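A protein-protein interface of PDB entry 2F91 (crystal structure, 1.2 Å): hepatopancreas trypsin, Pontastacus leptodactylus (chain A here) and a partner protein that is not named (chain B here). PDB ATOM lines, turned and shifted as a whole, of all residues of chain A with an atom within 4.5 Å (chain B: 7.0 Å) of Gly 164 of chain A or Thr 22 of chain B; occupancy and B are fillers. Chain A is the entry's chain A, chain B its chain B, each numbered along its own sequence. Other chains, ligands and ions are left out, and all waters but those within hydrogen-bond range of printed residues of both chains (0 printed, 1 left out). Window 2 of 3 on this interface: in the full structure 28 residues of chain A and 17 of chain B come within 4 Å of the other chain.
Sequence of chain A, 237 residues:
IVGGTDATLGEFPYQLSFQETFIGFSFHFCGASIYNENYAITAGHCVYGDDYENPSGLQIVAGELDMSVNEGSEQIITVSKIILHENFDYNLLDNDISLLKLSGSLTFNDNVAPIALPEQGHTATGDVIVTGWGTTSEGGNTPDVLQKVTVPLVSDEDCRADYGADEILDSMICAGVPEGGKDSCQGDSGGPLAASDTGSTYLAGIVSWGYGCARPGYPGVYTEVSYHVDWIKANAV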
ATOM      1  N   ARG A 160      -3.005 -26.794   7.952  1.00  0.00           N
ATOM      2  CA  ARG A 160      -4.292 -26.112   8.121  1.00  0.00           C
ATOM      3  C   ARG A 160      -5.166 -26.776   9.158  1.00  0.00           C
ATOM      4  O   ARG A 160      -5.984 -26.081   9.783  1.00  0.00           O
ATOM      5  CB  ARG A 160      -5.046 -26.069   6.779  1.00  0.00           C
ATOM      6  CG  ARG A 160      -4.430 -25.014   5.851  1.00  0.00           C
ATOM      7  CD  ARG A 160      -5.063 -25.124   4.469  1.00  0.00           C
ATOM      8  NE  ARG A 160      -4.348 -24.138   3.636  1.00  0.00           N
ATOM      9  CZ  ARG A 160      -3.937 -24.282   2.404  1.00  0.00           C
ATOM     10  NH1 ARG A 160      -4.127 -25.407   1.714  1.00  0.00           N
ATOM     11  NH2 ARG A 160      -3.297 -23.290   1.843  1.00  0.00           N
ATOM     12  N   ALA A 161      -4.989 -28.079   9.407  1.00  0.00           N
ATOM     13  CA  ALA A 161      -5.719 -28.673  10.546  1.00  0.00           C
ATOM     14  C   ALA A 161      -5.265 -28.048  11.856  1.00  0.00           C
ATOM     15  O   ALA A 161      -6.046 -28.020  12.805  1.00  0.00           O
ATOM     16  CB  ALA A 161      -5.558 -30.171  10.585  1.00  0.00           C
ATOM     17  N   ASP A 162      -4.034 -27.554  11.967  1.00  0.00           N
ATOM     18  CA  ASP A 162      -3.547 -26.986  13.199  1.00  0.00           C
ATOM     19  C   ASP A 162      -3.940 -25.523  13.347  1.00  0.00           C
ATOM     20  O   ASP A 162      -4.314 -25.004  14.408  1.00  0.00           O
ATOM     21  CB  ASP A 162      -2.007 -27.122  13.235  1.00  0.00           C
ATOM     22  CG  ASP A 162      -1.580 -28.560  12.953  1.00  0.00           C
ATOM     23  OD1 ASP A 162      -2.293 -29.450  13.458  1.00  0.00           O
ATOM     24  OD2 ASP A 162      -0.563 -28.698  12.245  1.00  0.00           O
ATOM     25  N   TYR A 163      -3.841 -24.794  12.233  1.00  0.00           N
ATOM     26  CA  TYR A 163      -3.897 -23.330  12.289  1.00  0.00           C
ATOM     27  C   TYR A 163      -5.111 -22.717  11.637  1.00  0.00           C
ATOM     28  O   TYR A 163      -5.445 -21.556  11.905  1.00  0.00           O
ATOM     29  CB  TYR A 163      -2.625 -22.785  11.672  1.00  0.00           C
ATOM     30  CG  TYR A 163      -1.353 -22.920  12.459  1.00  0.00           C
ATOM     31  CD1 TYR A 163      -1.228 -22.318  13.708  1.00  0.00           C
ATOM     32  CD2 TYR A 163      -0.273 -23.603  11.957  1.00  0.00           C
ATOM     33  CE1 TYR A 163      -0.052 -22.416  14.424  1.00  0.00           C
ATOM     34  CE2 TYR A 163       0.894 -23.695  12.662  1.00  0.00           C
ATOM     35  CZ  TYR A 163       0.987 -23.123  13.910  1.00  0.00           C
ATOM     36  OH  TYR A 163       2.169 -23.208  14.622  1.00  0.00           O
ATOM     37  N   GLY A 164      -5.842 -23.497  10.838  1.00  0.00           N
ATOM     38  CA  GLY A 164      -6.982 -22.987  10.103  1.00  0.00           C
ATOM     39  C   GLY A 164      -6.723 -22.846   8.635  1.00  0.00           C
ATOM     40  O   GLY A 164      -5.641 -22.491   8.203  1.00  0.00           O
ATOM     41  N   ALA A 165      -7.753 -23.140   7.844  1.00  0.00           N
ATOM     42  CA  ALA A 165      -7.616 -23.144   6.385  1.00  0.00           C
ATOM     43  C   ALA A 165      -7.043 -21.889   5.796  1.00  0.00           C
ATOM     44  O   ALA A 165      -6.095 -21.942   5.013  1.00  0.00           O
ATOM     45  CB  ALA A 165      -8.990 -23.445   5.758  1.00  0.00           C
ATOM     46  N   ASP A 166      -7.634 -20.739   6.144  1.00  0.00           N
ATOM     47  CA  ASP A 166      -7.248 -19.496   5.497  1.00  0.00           C
ATOM     48  C   ASP A 166      -6.054 -18.835   6.152  1.00  0.00           C
ATOM     49  O   ASP A 166      -5.489 -17.881   5.629  1.00  0.00           O
ATOM     50  CB  ASP A 166      -8.440 -18.510   5.441  1.00  0.00           C
ATOM     51  CG  ASP A 166      -9.567 -19.060   4.576  1.00  0.00           C
ATOM     52  OD1 ASP A 166      -9.308 -19.818   3.604  1.00  0.00           O
ATOM     53  OD2 ASP A 166     -10.758 -18.757   4.830  1.00  0.00           O
ATOM     54  N   GLU A 167      -5.621 -19.402   7.282  1.00  0.00           N
ATOM     55  CA  GLU A 167      -4.453 -18.893   8.015  1.00  0.00           C
ATOM     56  C   GLU A 167      -3.135 -19.319   7.384  1.00  0.00           C
ATOM     57  O   GLU A 167      -2.145 -18.616   7.463  1.00  0.00           O
ATOM     58  CB  GLU A 167      -4.504 -19.396   9.465  1.00  0.00           C
ATOM     59  CG  GLU A 167      -3.524 -18.665  10.390  1.00  0.00           C
ATOM     60  CD  GLU A 167      -3.942 -17.306  10.901  1.00  0.00           C
ATOM     61  OE1 GLU A 167      -5.058 -16.831  10.685  1.00  0.00           O
ATOM     62  OE2 GLU A 167      -3.082 -16.693  11.630  1.00  0.00           O
ATOM     63  N   ILE A 168      -3.146 -20.510   6.809  1.00  0.00           N
ATOM     64  CA  ILE A 168      -2.003 -21.019   6.060  1.00  0.00           C
ATOM     65  C   ILE A 168      -2.272 -20.782   4.590  1.00  0.00           C
ATOM     66  O   ILE A 168      -3.131 -21.436   4.003  1.00  0.00           O
ATOM     67  CB  ILE A 168      -1.737 -22.498   6.340  1.00  0.00           C
ATOM     68  CG1 ILE A 168      -1.581 -22.774   7.841  1.00  0.00           C
ATOM     69  CG2 ILE A 168      -0.555 -22.971   5.523  1.00  0.00           C
ATOM     70  CD1 ILE A 168      -0.384 -22.070   8.427  1.00  0.00           C
ATOM     71  N   GLN B   2     -11.213 -19.704  24.968  1.00  0.00           N
ATOM     72  CA  GLN B   2     -10.922 -21.023  24.395  1.00  0.00           C
ATOM     73  C   GLN B   2      -9.523 -21.027  23.758  1.00  0.00           C
ATOM     74  O   GLN B   2      -9.279 -21.715  22.768  1.00  0.00           O
ATOM     75  N   GLU B   3      -8.718 -20.249  24.407  1.00  0.00           N
ATOM     76  CA  GLU B   3      -7.466 -19.551  24.231  1.00  0.00           C
ATOM     77  C   GLU B   3      -7.645 -18.154  23.609  1.00  0.00           C
ATOM     78  O   GLU B   3      -7.178 -17.191  24.225  1.00  0.00           O
ATOM     79  CB  GLU B   3      -6.461 -20.335  23.376  1.00  0.00           C
ATOM     80  CG  GLU B   3      -5.330 -19.363  23.126  1.00  0.00           C
ATOM     81  CD  GLU B   3      -3.917 -19.854  23.112  1.00  0.00           C
ATOM     82  OE1 GLU B   3      -3.372 -20.006  21.992  1.00  0.00           O
ATOM     83  OE2 GLU B   3      -3.286 -20.053  24.171  1.00  0.00           O
ATOM     84  N   CYS B   4      -8.292 -17.994  22.449  1.00  0.00           N
ATOM     85  CA  CYS B   4      -8.614 -16.645  21.954  1.00  0.00           C
ATOM     86  C   CYS B   4      -9.770 -16.679  20.953  1.00  0.00           C
ATOM     87  O   CYS B   4     -10.141 -17.748  20.425  1.00  0.00           O
ATOM     88  CB  CYS B   4      -7.346 -16.023  21.367  1.00  0.00           C
ATOM     89  SG  CYS B   4      -6.562 -16.926  20.002  1.00  0.00           S
ATOM     90  N   PRO B   6     -11.096 -15.924  17.149  1.00  0.00           N
ATOM     91  CA  PRO B   6     -10.503 -15.719  15.805  1.00  0.00           C
ATOM     92  C   PRO B   6     -10.562 -14.282  15.341  1.00  0.00           C
ATOM     93  O   PRO B   6     -11.617 -13.643  15.387  1.00  0.00           O
ATOM     94  CB  PRO B   6     -11.378 -16.607  14.915  1.00  0.00           C
ATOM     95  CG  PRO B   6     -11.658 -17.759  15.848  1.00  0.00           C
ATOM     96  CD  PRO B   6     -12.014 -17.066  17.131  1.00  0.00           C
ATOM     97  N   CYS B  19      -5.189 -14.144  16.379  1.00  0.00           N
ATOM     98  CA  CYS B  19      -5.852 -15.361  16.796  1.00  0.00           C
ATOM     99  C   CYS B  19      -6.352 -16.106  15.555  1.00  0.00           C
ATOM    100  O   CYS B  19      -7.162 -15.546  14.802  1.00  0.00           O
ATOM    101  CB  CYS B  19      -7.008 -15.007  17.738  1.00  0.00           C
ATOM    102  SG  CYS B  19      -7.731 -16.542  18.385  1.00  0.00           S
ATOM    103  N   THR B  20      -5.878 -17.330  15.376  1.00  0.00           N
ATOM    104  CA  THR B  20      -6.217 -18.102  14.188  1.00  0.00           C
ATOM    105  C   THR B  20      -7.643 -18.605  14.222  1.00  0.00           C
ATOM    106  O   THR B  20      -8.324 -18.567  15.264  1.00  0.00           O
ATOM    107  CB  THR B  20      -5.339 -19.384  14.058  1.00  0.00           C
ATOM    108  OG1 THR B  20      -5.738 -20.221  15.156  1.00  0.00           O
ATOM    109  CG2 THR B  20      -3.876 -19.052  14.211  1.00  0.00           C
ATOM    110  N   PRO B  21      -8.195 -19.099  13.122  1.00  0.00           N
ATOM    111  CA  PRO B  21      -9.507 -19.723  13.100  1.00  0.00           C
ATOM    112  C   PRO B  21      -9.610 -20.886  14.085  1.00  0.00           C
ATOM    113  O   PRO B  21     -10.720 -21.197  14.535  1.00  0.00           O
ATOM    114  CB  PRO B  21      -9.686 -20.130  11.643  1.00  0.00           C
ATOM    115  CG  PRO B  21      -8.838 -19.179  10.865  1.00  0.00           C
ATOM    116  CD  PRO B  21      -7.646 -18.963  11.741  1.00  0.00           C
ATOM    117  N   THR B  22      -8.507 -21.509  14.457  1.00  0.00           N
ATOM    118  CA  THR B  22      -8.518 -22.601  15.421  1.00  0.00           C
ATOM    119  C   THR B  22      -8.347 -22.176  16.864  1.00  0.00           C
ATOM    120  O   THR B  22      -8.306 -23.027  17.768  1.00  0.00           O
ATOM    121  CB  THR B  22      -7.415 -23.640  15.094  1.00  0.00           C
ATOM    122  OG1 THR B  22      -6.137 -22.997  14.976  1.00  0.00           O
ATOM    123  CG2 THR B  22      -7.762 -24.312  13.789  1.00  0.00           C
ATOM    124  N   GLY B  23      -8.247 -20.881  17.119  1.00  0.00           N
ATOM    125  CA  GLY B  23      -8.280 -20.406  18.494  1.00  0.00           C
ATOM    126  C   GLY B  23      -6.929 -20.369  19.156  1.00  0.00           C
ATOM    127  O   GLY B  23      -6.936 -20.418  20.399  1.00  0.00           O
ATOM    128  N   VAL B  24      -5.807 -20.302  18.437  1.00  0.00           N
ATOM    129  CA  VAL B  24      -4.477 -20.189  19.036  1.00  0.00           C
ATOM    130  C   VAL B  24      -3.849 -18.890  18.533  1.00  0.00           C
ATOM    131  O   VAL B  24      -4.278 -18.260  17.544  1.00  0.00           O
ATOM    132  CB  VAL B  24      -3.543 -21.395  18.778  1.00  0.00           C
ATOM    133  CG1 VAL B  24      -4.144 -22.696  19.344  1.00  0.00           C
ATOM    134  CG2 VAL B  24      -3.250 -21.607  17.306  1.00  0.00           C
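O of Tyr 163 of chain A lies within hydrogen-bond range of OG1 of Thr 22 of chain B, 3.5 Å away.
OG1 of Thr 22 of chain B lies within hydrogen-bond range of O of Asp 162 of chain A (2.8 Å).
The backbone NH of Val 24 of chain B sits at hydrogen-bond distance from the side-chain hydroxyl of Thr 20 of chain B, 3.3 Å away.
N of Gly 23 of chain B sits at hydrogen-bond distance from OG1 of Thr 20 of chain B (3.3 Å).
The side-chain sulfur (SG) of Cys 4 of chain B is disulfide-bonded to the side-chain sulfur (SG) of Cys 19 of chain B (2.0 Å).
OG1 of Thr 20 of chain B is in hydrogen-bond range of OG1 of Thr 22 of chain B (2.8 Å).
Thr 20 of chain B touches Tyr 163 of chain A.
CD of Pro 21 of chain B touches O of Tyr 163 of chain A (3.4 Å).
Gly 164 of chain A touches Thr 22 of chain B (N to CG2, 3.6 Å).
Glu 167 of chain A touches Thr 20 of chain B.
Glu 167 of chain A touches Pro 21 of chain B (OE1 to CD, 3.5 Å).
Of chain B, only Thr 22 (3.6 Å) comes within 4 Å of Gly 164 of chain A.
Of chain A, only Asp 162, Tyr 163 and Gly 164 come within 4 Å of Thr 22 of chain B.
Of the printed residues of chain B, Glu 167 of chain A touches Thr 20 (3.6 Å) and Pro 21 (3.5 Å).
Printed residues of chain B within 4 Å of Asp 162 of chain A: Thr 22.
Of the printed residues of chain A, Thr 20 of chain B touches Tyr 163 and Glu 167.
Printed residues of chain A within 4 Å of Pro 21 of chain B: Tyr 163 (3.4 Å) and Glu 167 (3.5 Å).
Val 24 of chain B touches none of the printed residues of chain A.
The nearest residue of chain A that does not touch Thr 22 of chain B is Ala 161 of chain A (4.2 Å).
Printed residues of chain B that touch a printed residue of chain A: Thr 20, Pro 21 and Thr 22.
Along chain B the printed residues that touch a printed residue of chain A span positions 20 to 22.
Of the 9 printed residues of chain A, 4 touch a printed residue of chain B.
Among the printed residues, 7 pairs touch across the chains.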
